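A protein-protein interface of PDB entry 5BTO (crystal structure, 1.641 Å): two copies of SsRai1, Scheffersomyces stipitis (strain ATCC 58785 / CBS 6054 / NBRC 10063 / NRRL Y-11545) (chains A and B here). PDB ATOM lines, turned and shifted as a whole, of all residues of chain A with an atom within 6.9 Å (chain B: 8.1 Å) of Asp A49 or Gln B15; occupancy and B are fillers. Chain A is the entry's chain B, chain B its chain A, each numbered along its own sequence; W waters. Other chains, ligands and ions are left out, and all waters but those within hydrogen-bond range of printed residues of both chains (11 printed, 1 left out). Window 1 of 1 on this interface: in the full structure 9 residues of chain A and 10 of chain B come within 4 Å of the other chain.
Of the 17 printed residues of chain B, 9 touch a printed residue of chain A. Among the printed residues, 16 pairs touch across the chains.
Of the printed residues of chain B, Lys A45 touches Leu B12, Ser B16 and Trp B346. Of the printed residues of chain B, Asp A49 touches Ser B13, Gln B15 and Ser B16. Of the printed residues of chain A, Thr B11 touches Ile A46. Leu B14 touches none of the printed residues of chain A. Gln B15 touches four residues of chain A. Of the printed residues of chain A, Ser B327 touches Lys A193 (2.4 Å) and Asp A197 (2.8 Å). The nearest residue of chain B that does not touch Asp A49 is Leu B12 (4.5 Å).
No position is printed for both chains.
The backbone NH (N) of Leu B12 sits at hydrogen-bond distance from the backbone carbonyl oxygen (O) of Phe B371 (2.9 Å). The side-chain hydroxyl (OG) of Ser B327 is in hydrogen-bond range of the guanidinium group (NH2) of Arg B17. O of Ile A46 sits close to OD1 of Asn A51 (3.2 Å). NZ of Lys A193 lies within hydrogen-bond range of O of Asp A197, at 2.9 Å. The side-chain amino group (NZ) of Lys A193 lies within hydrogen-bond range of the side-chain amide oxygen (OE1) of Gln A202, 3.4 Å away. OD2 of Asp A43 is in hydrogen-bond range of N of Lys A45 (3.2 Å).
Lys A45 touches Leu B12 (CE to CD1, 3.5 Å). Ser B16 touches Lys A45 (OG to CE, 3.5 Å). Trp B346 touches Lys A45 (CD1 to CD, 3.7 Å). Ile A46 touches Thr B11. CD1 of Ile A46 touches N of Ser B13 (3.9 Å). Asp A49 touches Ser B13. Gln B15 touches Glu A50. OE1 of Gln B15 touches O of Pro A192 (3.7 Å). Lys A193 touches Gln B15. Asp A197 touches Thr B335 (OD1 to CG2, 3.998 Å).
The backbone NH (N) of Ser B327 lies close to the side-chain amino group (NZ) of Lys A193 (2.4 Å). O of Asp A49 lies close to OE1 of Gln B15 (2.9 Å). OG of Ser B327 lies within hydrogen-bond range of O of Asp A197 (2.8 Å). The side-chain hydroxyl (OG) of Ser B13 lies within hydrogen-bond range of the side-chain carboxylate (OE2) of Glu A50 (2.6 Å). The guanidinium group (NE) of Arg B17 is in salt-bridge range of the side-chain carboxylate (OD1) of Asp A197 (3.8 Å). The side-chain hydroxyl of Ser B16 sits at hydrogen-bond distance from the side-chain carboxylate of Asp A49.
Water W8 bridges O of Ala B342 (2.7 Å) and NZ of Lys A45 (3.1 Å). Water W7 lies within hydrogen-bond range of OD2 of Asp A49 (2.7 Å) and N of Ser B13 (2.9 Å). Water W9 lies within hydrogen-bond range of the side-chain carboxylate of Glu A50 (2.8 Å) and the backbone NH of Leu B14 (2.9 Å). Water W11 bridges the backbone carbonyl oxygen of Thr B11 (2.8 Å) and the side-chain carboxylate of Asp A43 (3.3 Å). Water W1 lies within hydrogen-bond range of the side-chain carboxylate of Asp A49 (2.9 Å) and the backbone NH of Arg B17 (2.9 Å). Water W10 lies within hydrogen-bond range of NZ of Lys B338, OG1 of Thr B335 and OD1 of Asp A197.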
ATOM      1  N   ASP A  43     -29.016  20.441  18.226  1.00  0.00           N
ATOM      2  CA  ASP A  43     -29.211  19.834  19.534  1.00  0.00           C
ATOM      3  C   ASP A  43     -29.658  20.885  20.544  1.00  0.00           C
ATOM      4  O   ASP A  43     -29.006  21.909  20.691  1.00  0.00           O
ATOM      5  CB  ASP A  43     -27.925  19.153  20.004  1.00  0.00           C
ATOM      6  CG  ASP A  43     -28.081  18.500  21.369  1.00  0.00           C
ATOM      7  OD1 ASP A  43     -28.655  17.390  21.448  1.00  0.00           O
ATOM      8  OD2 ASP A  43     -27.634  19.098  22.366  1.00  0.00           O
ATOM      9  N   GLN A  44     -30.777  20.637  21.224  1.00  0.00           N
ATOM     10  CA  GLN A  44     -31.365  21.625  22.123  1.00  0.00           C
ATOM     11  C   GLN A  44     -30.428  22.041  23.257  1.00  0.00           C
ATOM     12  O   GLN A  44     -30.339  23.215  23.602  1.00  0.00           O
ATOM     13  CB  GLN A  44     -32.683  21.107  22.712  1.00  0.00           C
ATOM     14  CG  GLN A  44     -33.765  20.893  21.684  1.00  0.00           C
ATOM     15  CD  GLN A  44     -33.980  22.130  20.852  1.00  0.00           C
ATOM     16  OE1 GLN A  44     -34.615  23.092  21.300  1.00  0.00           O
ATOM     17  NE2 GLN A  44     -33.429  22.130  19.641  1.00  0.00           N
ATOM     18  N   LYS A  45     -29.736  21.073  23.842  1.00  0.00           N
ATOM     19  CA  LYS A  45     -28.870  21.375  24.968  1.00  0.00           C
ATOM     20  C   LYS A  45     -27.698  22.255  24.525  1.00  0.00           C
ATOM     21  O   LYS A  45     -27.385  23.246  25.176  1.00  0.00           O
ATOM     22  CB  LYS A  45     -28.370  20.090  25.627  1.00  0.00           C
ATOM     23  CG  LYS A  45     -27.641  20.337  26.934  1.00  0.00           C
ATOM     24  CD  LYS A  45     -27.168  19.026  27.555  1.00  0.00           C
ATOM     25  CE  LYS A  45     -26.447  19.279  28.866  1.00  0.00           C
ATOM     26  NZ  LYS A  45     -27.356  19.855  29.902  1.00  0.00           N
ATOM     27  N   ILE A  46     -27.062  21.912  23.407  1.00  0.00           N
ATOM     28  CA  ILE A  46     -25.887  22.668  22.994  1.00  0.00           C
ATOM     29  C   ILE A  46     -26.259  24.072  22.504  1.00  0.00           C
ATOM     30  O   ILE A  46     -25.499  25.020  22.683  1.00  0.00           O
ATOM     31  CB  ILE A  46     -25.010  21.889  21.993  1.00  0.00           C
ATOM     32  CG1 ILE A  46     -23.542  22.324  22.122  1.00  0.00           C
ATOM     33  CG2 ILE A  46     -25.549  22.005  20.591  1.00  0.00           C
ATOM     34  CD1 ILE A  46     -22.553  21.293  21.601  1.00  0.00           C
ATOM     35  N   VAL A  47     -27.445  24.202  21.913  1.00  0.00           N
ATOM     36  CA  VAL A  47     -27.943  25.501  21.492  1.00  0.00           C
ATOM     37  C   VAL A  47     -28.096  26.428  22.705  1.00  0.00           C
ATOM     38  O   VAL A  47     -27.674  27.586  22.678  1.00  0.00           O
ATOM     39  CB  VAL A  47     -29.272  25.338  20.697  1.00  0.00           C
ATOM     40  CG1 VAL A  47     -29.990  26.668  20.528  1.00  0.00           C
ATOM     41  CG2 VAL A  47     -28.985  24.692  19.353  1.00  0.00           C
ATOM     42  N   LYS A  48     -28.667  25.903  23.787  1.00  0.00           N
ATOM     43  CA  LYS A  48     -28.831  26.675  25.014  1.00  0.00           C
ATOM     44  C   LYS A  48     -27.505  26.902  25.763  1.00  0.00           C
ATOM     45  O   LYS A  48     -27.303  27.959  26.355  1.00  0.00           O
ATOM     46  CB  LYS A  48     -29.868  26.000  25.929  1.00  0.00           C
ATOM     47  CG  LYS A  48     -31.309  26.023  25.365  1.00  0.00           C
ATOM     48  CD  LYS A  48     -31.961  27.368  25.607  1.00  0.00           C
ATOM     49  CE  LYS A  48     -33.458  27.358  25.323  1.00  0.00           C
ATOM     50  NZ  LYS A  48     -33.750  27.119  23.892  1.00  0.00           N
ATOM     51  N   ASP A  49     -26.596  25.933  25.703  1.00  0.00           N
ATOM     52  CA  ASP A  49     -25.359  25.999  26.492  1.00  0.00           C
ATOM     53  C   ASP A  49     -24.323  26.938  25.882  1.00  0.00           C
ATOM     54  O   ASP A  49     -23.528  27.542  26.607  1.00  0.00           O
ATOM     55  CB  ASP A  49     -24.719  24.617  26.629  1.00  0.00           C
ATOM     56  CG  ASP A  49     -25.363  23.761  27.712  1.00  0.00           C
ATOM     57  OD1 ASP A  49     -26.199  24.267  28.497  1.00  0.00           O
ATOM     58  OD2 ASP A  49     -25.006  22.569  27.778  1.00  0.00           O
ATOM     59  N   GLU A  50     -24.306  27.070  24.557  1.00  0.00           N
ATOM     60  CA  GLU A  50     -23.237  27.869  23.961  1.00  0.00           C
ATOM     61  C   GLU A  50     -23.612  28.694  22.727  1.00  0.00           C
ATOM     62  O   GLU A  50     -22.730  29.232  22.068  1.00  0.00           O
ATOM     63  CB  GLU A  50     -21.995  27.003  23.677  1.00  0.00           C
ATOM     64  CG  GLU A  50     -22.165  25.984  22.542  1.00  0.00           C
ATOM     65  CD  GLU A  50     -20.926  25.129  22.305  1.00  0.00           C
ATOM     66  OE1 GLU A  50     -20.746  24.634  21.175  1.00  0.00           O
ATOM     67  OE2 GLU A  50     -20.126  24.933  23.246  1.00  0.00           O
ATOM     68  N   ASN A  51     -24.904  28.812  22.425  1.00  0.00           N
ATOM     69  CA  ASN A  51     -25.310  29.612  21.266  1.00  0.00           C
ATOM     70  C   ASN A  51     -26.217  30.808  21.550  1.00  0.00           C
ATOM     71  O   ASN A  51     -26.767  31.403  20.627  1.00  0.00           O
ATOM     72  CB  ASN A  51     -25.927  28.724  20.183  1.00  0.00           C
ATOM     73  CG  ASN A  51     -24.913  27.759  19.579  1.00  0.00           C
ATOM     74  OD1 ASN A  51     -24.741  26.629  20.059  1.00  0.00           O
ATOM     75  ND2 ASN A  51     -24.231  28.200  18.530  1.00  0.00           N
ATOM     76  N   VAL A  52     -26.396  31.161  22.817  1.00  0.00           N
ATOM     77  CA  VAL A  52     -27.117  32.393  23.126  1.00  0.00           C
ATOM     78  C   VAL A  52     -26.377  33.187  24.200  1.00  0.00           C
ATOM     79  O   VAL A  52     -25.855  32.626  25.152  1.00  0.00           O
ATOM     80  CB  VAL A  52     -28.580  32.137  23.535  1.00  0.00           C
ATOM     81  CG1 VAL A  52     -28.641  31.361  24.842  1.00  0.00           C
ATOM     82  CG2 VAL A  52     -29.335  33.463  23.652  1.00  0.00           C
ATOM     83  N   TYR A  54     -25.762  36.526  27.051  1.00  0.00           N
ATOM     84  CA  TYR A  54     -26.420  37.098  28.217  1.00  0.00           C
ATOM     85  C   TYR A  54     -26.121  38.583  28.320  1.00  0.00           C
ATOM     86  O   TYR A  54     -24.974  38.993  28.177  1.00  0.00           O
ATOM     87  CB  TYR A  54     -25.920  36.401  29.483  1.00  0.00           C
ATOM     88  CG  TYR A  54     -26.301  34.946  29.547  1.00  0.00           C
ATOM     89  CD1 TYR A  54     -25.584  33.986  28.847  1.00  0.00           C
ATOM     90  CD2 TYR A  54     -27.388  34.533  30.308  1.00  0.00           C
ATOM     91  CE1 TYR A  54     -25.947  32.630  28.903  1.00  0.00           C
ATOM     92  CE2 TYR A  54     -27.755  33.194  30.369  1.00  0.00           C
ATOM     93  CZ  TYR A  54     -27.035  32.253  29.661  1.00  0.00           C
ATOM     94  OH  TYR A  54     -27.402  30.931  29.730  1.00  0.00           O
ATOM     95  N   PRO A 192     -20.879  35.540  26.976  1.00  0.00           N
ATOM     96  CA  PRO A 192     -21.197  34.211  26.420  1.00  0.00           C
ATOM     97  C   PRO A 192     -21.808  33.244  27.437  1.00  0.00           C
ATOM     98  O   PRO A 192     -22.425  32.246  27.056  1.00  0.00           O
ATOM     99  CB  PRO A 192     -19.833  33.694  25.962  1.00  0.00           C
ATOM    100  CG  PRO A 192     -18.861  34.371  26.887  1.00  0.00           C
ATOM    101  CD  PRO A 192     -19.427  35.739  27.138  1.00  0.00           C
ATOM    102  N   LYS A 193     -21.617  33.529  28.719  1.00  0.00           N
ATOM    103  CA  LYS A 193     -22.172  32.713  29.790  1.00  0.00           C
ATOM    104  C   LYS A 193     -22.577  33.654  30.904  1.00  0.00           C
ATOM    105  O   LYS A 193     -22.240  34.840  30.854  1.00  0.00           O
ATOM    106  CB  LYS A 193     -21.127  31.731  30.323  1.00  0.00           C
ATOM    107  CG  LYS A 193     -20.729  30.627  29.367  1.00  0.00           C
ATOM    108  CD  LYS A 193     -19.529  29.857  29.914  1.00  0.00           C
ATOM    109  CE  LYS A 193     -18.285  30.735  29.919  1.00  0.00           C
ATOM    110  NZ  LYS A 193     -17.070  30.000  30.362  1.00  0.00           N
ATOM    111  N   PRO A 194     -23.302  33.141  31.911  1.00  0.00           N
ATOM    112  CA  PRO A 194     -23.570  33.962  33.092  1.00  0.00           C
ATOM    113  C   PRO A 194     -22.256  34.428  33.692  1.00  0.00           C
ATOM    114  O   PRO A 194     -21.250  33.721  33.612  1.00  0.00           O
ATOM    115  CB  PRO A 194     -24.275  32.985  34.043  1.00  0.00           C
ATOM    116  CG  PRO A 194     -24.905  31.975  33.128  1.00  0.00           C
ATOM    117  CD  PRO A 194     -23.915  31.803  32.016  1.00  0.00           C
ATOM    118  N   ASP A 197     -19.795  32.299  35.584  1.00  0.00           N
ATOM    119  CA  ASP A 197     -19.143  31.210  34.868  1.00  0.00           C
ATOM    120  C   ASP A 197     -18.177  31.704  33.791  1.00  0.00           C
ATOM    121  O   ASP A 197     -17.667  30.913  33.004  1.00  0.00           O
ATOM    122  CB  ASP A 197     -20.185  30.241  34.290  1.00  0.00           C
ATOM    123  CG  ASP A 197     -21.064  29.618  35.369  1.00  0.00           C
ATOM    124  OD1 ASP A 197     -20.525  28.879  36.233  1.00  0.00           O
ATOM    125  OD2 ASP A 197     -22.295  29.864  35.353  1.00  0.00           O
ATOM    126  N   GLN A 202     -12.769  36.827  29.469  1.00  0.00           N
ATOM    127  CA  GLN A 202     -14.007  36.843  28.700  1.00  0.00           C
ATOM    128  C   GLN A 202     -14.825  38.097  28.980  1.00  0.00           C
ATOM    129  O   GLN A 202     -15.498  38.620  28.092  1.00  0.00           O
ATOM    130  CB  GLN A 202     -14.834  35.590  28.978  1.00  0.00           C
ATOM    131  CG  GLN A 202     -14.308  34.355  28.276  1.00  0.00           C
ATOM    132  CD  GLN A 202     -15.101  33.114  28.620  1.00  0.00           C
ATOM    133  OE1 GLN A 202     -15.341  32.826  29.796  1.00  0.00           O
ATOM    134  NE2 GLN A 202     -15.521  32.374  27.597  1.00  0.00           N
ATOM    135  N   ILE A 243     -31.752  31.390  31.836  1.00  0.00           N
ATOM    136  CA  ILE A 243     -32.620  30.424  31.183  1.00  0.00           C
ATOM    137  C   ILE A 243     -33.159  29.488  32.254  1.00  0.00           C
ATOM    138  O   ILE A 243     -32.385  28.795  32.909  1.00  0.00           O
ATOM    139  CB  ILE A 243     -31.851  29.601  30.146  1.00  0.00           C
ATOM    140  CG1 ILE A 243     -31.225  30.512  29.084  1.00  0.00           C
ATOM    141  CG2 ILE A 243     -32.768  28.585  29.493  1.00  0.00           C
ATOM    142  CD1 ILE A 243     -30.251  29.799  28.185  1.00  0.00           C
ATOM    143  N   THR B  11     -22.329  15.610  21.360  1.00  0.00           N
ATOM    144  CA  THR B  11     -21.369  16.582  21.895  1.00  0.00           C
ATOM    145  C   THR B  11     -21.945  17.344  23.075  1.00  0.00           C
ATOM    146  O   THR B  11     -23.103  17.742  23.063  1.00  0.00           O
ATOM    147  CB  THR B  11     -20.920  17.598  20.806  1.00  0.00           C
ATOM    148  OG1 THR B  11     -20.273  16.894  19.740  1.00  0.00           O
ATOM    149  CG2 THR B  11     -19.960  18.633  21.388  1.00  0.00           C
ATOM    150  N   LEU B  12     -21.126  17.528  24.113  1.00  0.00           N
ATOM    151  CA  LEU B  12     -21.503  18.339  25.259  1.00  0.00           C
ATOM    152  C   LEU B  12     -20.682  19.627  25.247  1.00  0.00           C
ATOM    153  O   LEU B  12     -19.461  19.576  25.152  1.00  0.00           O
ATOM    154  CB  LEU B  12     -21.242  17.567  26.569  1.00  0.00           C
ATOM    155  CG  LEU B  12     -21.581  18.316  27.860  1.00  0.00           C
ATOM    156  CD1 LEU B  12     -23.081  18.546  28.023  1.00  0.00           C
ATOM    157  CD2 LEU B  12     -21.025  17.575  29.089  1.00  0.00           C
ATOM    158  N   SER B  13     -21.354  20.773  25.328  1.00  0.00           N
ATOM    159  CA  SER B  13     -20.664  22.065  25.393  1.00  0.00           C
ATOM    160  C   SER B  13     -19.754  22.140  26.608  1.00  0.00           C
ATOM    161  O   SER B  13     -20.166  21.781  27.707  1.00  0.00           O
ATOM    162  CB  SER B  13     -21.650  23.217  25.516  1.00  0.00           C
ATOM    163  OG  SER B  13     -20.935  24.439  25.670  1.00  0.00           O
ATOM    164  N   LEU B  14     -18.539  22.636  26.413  1.00  0.00           N
ATOM    165  CA  LEU B  14     -17.637  22.857  27.545  1.00  0.00           C
ATOM    166  C   LEU B  14     -18.208  23.900  28.500  1.00  0.00           C
ATOM    167  O   LEU B  14     -17.754  24.023  29.645  1.00  0.00           O
ATOM    168  CB  LEU B  14     -16.258  23.326  27.065  1.00  0.00           C
ATOM    169  CG  LEU B  14     -15.445  22.339  26.231  1.00  0.00           C
ATOM    170  CD1 LEU B  14     -14.062  22.915  25.974  1.00  0.00           C
ATOM    171  CD2 LEU B  14     -15.346  20.980  26.917  1.00  0.00           C
ATOM    172  N   GLN B  15     -19.178  24.677  28.018  1.00  0.00           N
ATOM    173  CA  GLN B  15     -19.820  25.708  28.826  1.00  0.00           C
ATOM    174  C   GLN B  15     -20.961  25.169  29.693  1.00  0.00           C
ATOM    175  O   GLN B  15     -21.569  25.921  30.438  1.00  0.00           O
ATOM    176  CB  GLN B  15     -20.349  26.843  27.931  1.00  0.00           C
ATOM    177  CG  GLN B  15     -19.268  27.555  27.157  1.00  0.00           C
ATOM    178  CD  GLN B  15     -19.779  28.803  26.451  1.00  0.00           C
ATOM    179  OE1 GLN B  15     -20.979  28.943  26.183  1.00  0.00           O
ATOM    180  NE2 GLN B  15     -18.874  29.717  26.144  1.00  0.00           N
ATOM    181  N   SER B  16     -21.257  23.876  29.588  1.00  0.00           N
ATOM    182  CA  SER B  16     -22.426  23.329  30.284  1.00  0.00           C
ATOM    183  C   SER B  16     -22.204  23.385  31.797  1.00  0.00           C
ATOM    184  O   SER B  16     -21.120  23.066  32.273  1.00  0.00           O
ATOM    185  CB  SER B  16     -22.716  21.896  29.838  1.00  0.00           C
ATOM    186  OG  SER B  16     -24.042  21.537  30.175  1.00  0.00           O
ATOM    187  N   ARG B  17     -23.229  23.792  32.543  1.00  0.00           N
ATOM    188  CA  ARG B  17     -23.102  23.929  33.996  1.00  0.00           C
ATOM    189  C   ARG B  17     -24.377  23.477  34.686  1.00  0.00           C
ATOM    190  O   ARG B  17     -25.472  23.944  34.347  1.00  0.00           O
ATOM    191  CB  ARG B  17     -22.830  25.390  34.394  1.00  0.00           C
ATOM    192  CG  ARG B  17     -21.536  26.003  33.870  1.00  0.00           C
ATOM    193  CD  ARG B  17     -20.292  25.424  34.527  1.00  0.00           C
ATOM    194  NE  ARG B  17     -19.062  26.078  34.060  1.00  0.00           N
ATOM    195  CZ  ARG B  17     -18.363  25.683  32.999  1.00  0.00           C
ATOM    196  NH1 ARG B  17     -18.768  24.637  32.270  1.00  0.00           N
ATOM    197  NH2 ARG B  17     -17.255  26.331  32.658  1.00  0.00           N
ATOM    198  N   ALA B  18     -24.241  22.574  35.654  1.00  0.00           N
ATOM    199  CA  ALA B  18     -25.373  22.196  36.485  1.00  0.00           C
ATOM    200  C   ALA B  18     -25.608  23.250  37.562  1.00  0.00           C
ATOM    201  O   ALA B  18     -24.711  24.029  37.897  1.00  0.00           O
ATOM    202  CB  ALA B  18     -25.137  20.826  37.116  1.00  0.00           C
ATOM    203  N   LEU B 124     -11.101  19.297  34.360  1.00  0.00           N
ATOM    204  CA  LEU B 124     -10.992  19.598  32.924  1.00  0.00           C
ATOM    205  C   LEU B 124     -11.040  21.086  32.522  1.00  0.00           C
ATOM    206  O   LEU B 124     -10.247  21.516  31.690  1.00  0.00           O
ATOM    207  CB  LEU B 124     -12.038  18.765  32.137  1.00  0.00           C
ATOM    208  CG  LEU B 124     -12.070  18.870  30.606  1.00  0.00           C
ATOM    209  CD1 LEU B 124     -12.599  17.572  29.976  1.00  0.00           C
ATOM    210  CD2 LEU B 124     -12.912  20.071  30.137  1.00  0.00           C
ATOM    211  N   SER B 327     -14.898  28.897  30.526  1.00  0.00           N
ATOM    212  CA  SER B 327     -14.054  28.834  31.714  1.00  0.00           C
ATOM    213  C   SER B 327     -12.725  28.166  31.420  1.00  0.00           C
ATOM    214  O   SER B 327     -12.611  26.931  31.430  1.00  0.00           O
ATOM    215  CB  SER B 327     -14.756  28.103  32.866  1.00  0.00           C
ATOM    216  OG  SER B 327     -15.775  28.896  33.443  1.00  0.00           O
ATOM    217  N   THR B 335     -17.135  26.483  39.951  1.00  0.00           N
ATOM    218  CA  THR B 335     -17.377  26.315  38.523  1.00  0.00           C
ATOM    219  C   THR B 335     -17.018  24.894  38.088  1.00  0.00           C
ATOM    220  O   THR B 335     -17.750  24.253  37.315  1.00  0.00           O
ATOM    221  CB  THR B 335     -16.553  27.333  37.703  1.00  0.00           C
ATOM    222  OG1 THR B 335     -16.854  28.654  38.156  1.00  0.00           O
ATOM    223  CG2 THR B 335     -16.883  27.230  36.233  1.00  0.00           C
ATOM    224  N   LYS B 338     -19.748  22.541  39.138  1.00  0.00           N
ATOM    225  CA  LYS B 338     -20.930  22.674  38.280  1.00  0.00           C
ATOM    226  C   LYS B 338     -20.717  22.005  36.918  1.00  0.00           C
ATOM    227  O   LYS B 338     -21.643  21.392  36.367  1.00  0.00           O
ATOM    228  CB  LYS B 338     -21.314  24.150  38.104  1.00  0.00           C
ATOM    229  CG  LYS B 338     -21.833  24.826  39.371  1.00  0.00           C
ATOM    230  CD  LYS B 338     -22.018  26.315  39.136  1.00  0.00           C
ATOM    231  CE  LYS B 338     -22.321  27.058  40.420  1.00  0.00           C
ATOM    232  NZ  LYS B 338     -22.356  28.537  40.221  1.00  0.00           N
ATOM    233  N   TRP B 339     -19.513  22.130  36.356  1.00  0.00           N
ATOM    234  CA  TRP B 339     -19.184  21.396  35.128  1.00  0.00           C
ATOM    235  C   TRP B 339     -19.273  19.879  35.359  1.00  0.00           C
ATOM    236  O   TRP B 339     -19.854  19.131  34.572  1.00  0.00           O
ATOM    237  CB  TRP B 339     -17.788  21.787  34.623  1.00  0.00           C
ATOM    238  CG  TRP B 339     -17.130  20.746  33.761  1.00  0.00           C
ATOM    239  CD1 TRP B 339     -16.105  19.908  34.117  1.00  0.00           C
ATOM    240  CD2 TRP B 339     -17.466  20.411  32.405  1.00  0.00           C
ATOM    241  NE1 TRP B 339     -15.770  19.091  33.063  1.00  0.00           N
ATOM    242  CE2 TRP B 339     -16.587  19.379  31.999  1.00  0.00           C
ATOM    243  CE3 TRP B 339     -18.410  20.897  31.490  1.00  0.00           C
ATOM    244  CZ2 TRP B 339     -16.628  18.813  30.727  1.00  0.00           C
ATOM    245  CZ3 TRP B 339     -18.451  20.339  30.218  1.00  0.00           C
ATOM    246  CH2 TRP B 339     -17.561  19.303  29.848  1.00  0.00           C
ATOM    247  N   ALA B 342     -22.689  18.693  35.452  1.00  0.00           N
ATOM    248  CA  ALA B 342     -23.294  18.684  34.115  1.00  0.00           C
ATOM    249  C   ALA B 342     -22.897  17.432  33.337  1.00  0.00           C
ATOM    250  O   ALA B 342     -23.725  16.819  32.643  1.00  0.00           O
ATOM    251  CB  ALA B 342     -22.898  19.967  33.320  1.00  0.00           C
ATOM    252  N   TRP B 346     -25.417  14.482  32.155  1.00  0.00           N
ATOM    253  CA  TRP B 346     -25.497  14.248  30.720  1.00  0.00           C
ATOM    254  C   TRP B 346     -25.264  12.771  30.384  1.00  0.00           C
ATOM    255  O   TRP B 346     -26.016  12.176  29.612  1.00  0.00           O
ATOM    256  CB  TRP B 346     -24.471  15.133  30.004  1.00  0.00           C
ATOM    257  CG  TRP B 346     -24.546  15.155  28.510  1.00  0.00           C
ATOM    258  CD1 TRP B 346     -25.565  15.650  27.744  1.00  0.00           C
ATOM    259  CD2 TRP B 346     -23.531  14.719  27.599  1.00  0.00           C
ATOM    260  NE1 TRP B 346     -25.246  15.535  26.408  1.00  0.00           N
ATOM    261  CE2 TRP B 346     -24.003  14.971  26.291  1.00  0.00           C
ATOM    262  CE3 TRP B 346     -22.269  14.134  27.761  1.00  0.00           C
ATOM    263  CZ2 TRP B 346     -23.260  14.659  25.151  1.00  0.00           C
ATOM    264  CZ3 TRP B 346     -21.525  13.827  26.633  1.00  0.00           C
ATOM    265  CH2 TRP B 346     -22.031  14.088  25.335  1.00  0.00           C
ATOM    266  N   ARG B 369     -10.901  20.997  21.297  1.00  0.00           N
ATOM    267  CA  ARG B 369     -11.619  21.341  22.517  1.00  0.00           C
ATOM    268  C   ARG B 369     -13.083  20.927  22.454  1.00  0.00           C
ATOM    269  O   ARG B 369     -13.986  21.720  22.717  1.00  0.00           O
ATOM    270  CB  ARG B 369     -11.459  22.822  22.858  1.00  0.00           C
ATOM    271  CG  ARG B 369     -10.071  23.145  23.376  1.00  0.00           C
ATOM    272  CD  ARG B 369      -9.977  24.553  23.924  1.00  0.00           C
ATOM    273  NE  ARG B 369      -8.632  24.856  24.401  1.00  0.00           N
ATOM    274  CZ  ARG B 369      -8.310  25.978  25.033  1.00  0.00           C
ATOM    275  NH1 ARG B 369      -9.243  26.891  25.263  1.00  0.00           N
ATOM    276  NH2 ARG B 369      -7.063  26.184  25.436  1.00  0.00           N
ATOM    277  N   PHE B 371     -15.935  17.884  23.667  1.00  0.00           N
ATOM    278  CA  PHE B 371     -16.242  16.807  24.598  1.00  0.00           C
ATOM    279  C   PHE B 371     -17.360  15.988  23.969  1.00  0.00           C
ATOM    280  O   PHE B 371     -18.447  16.511  23.717  1.00  0.00           O
ATOM    281  CB  PHE B 371     -16.705  17.401  25.924  1.00  0.00           C
ATOM    282  CG  PHE B 371     -16.748  16.408  27.058  1.00  0.00           C
ATOM    283  CD1 PHE B 371     -17.856  15.595  27.238  1.00  0.00           C
ATOM    284  CD2 PHE B 371     -15.689  16.299  27.944  1.00  0.00           C
ATOM    285  CE1 PHE B 371     -17.914  14.686  28.289  1.00  0.00           C
ATOM    286  CE2 PHE B 371     -15.734  15.389  28.985  1.00  0.00           C
ATOM    287  CZ  PHE B 371     -16.849  14.578  29.165  1.00  0.00           C
HETATM  288  O   HOH W   1     -25.487  25.083  31.195  1.00  0.00           O
HETATM  289  O   HOH W   2     -16.563  27.154  29.313  1.00  0.00           O
HETATM  290  O   HOH W   3     -16.329  29.775  26.908  1.00  0.00           O
HETATM  291  O   HOH W   4     -27.215  16.621  24.372  1.00  0.00           O
HETATM  292  O   HOH W   5     -25.226  18.767  24.551  1.00  0.00           O
HETATM  293  O   HOH W   6     -25.901  21.305  32.185  1.00  0.00           O
HETATM  294  O   HOH W   7     -24.208  21.109  25.594  1.00  0.00           O
HETATM  295  O   HOH W   8     -26.123  17.968  31.995  1.00  0.00           O
HETATM  296  O   HOH W   9     -17.725  23.503  23.748  1.00  0.00           O
HETATM  297  O   HOH W  10     -19.616  29.267  39.337  1.00  0.00           O
HETATM  298  O   HOH W  11     -24.743  18.502  20.873  1.00  0.00           O
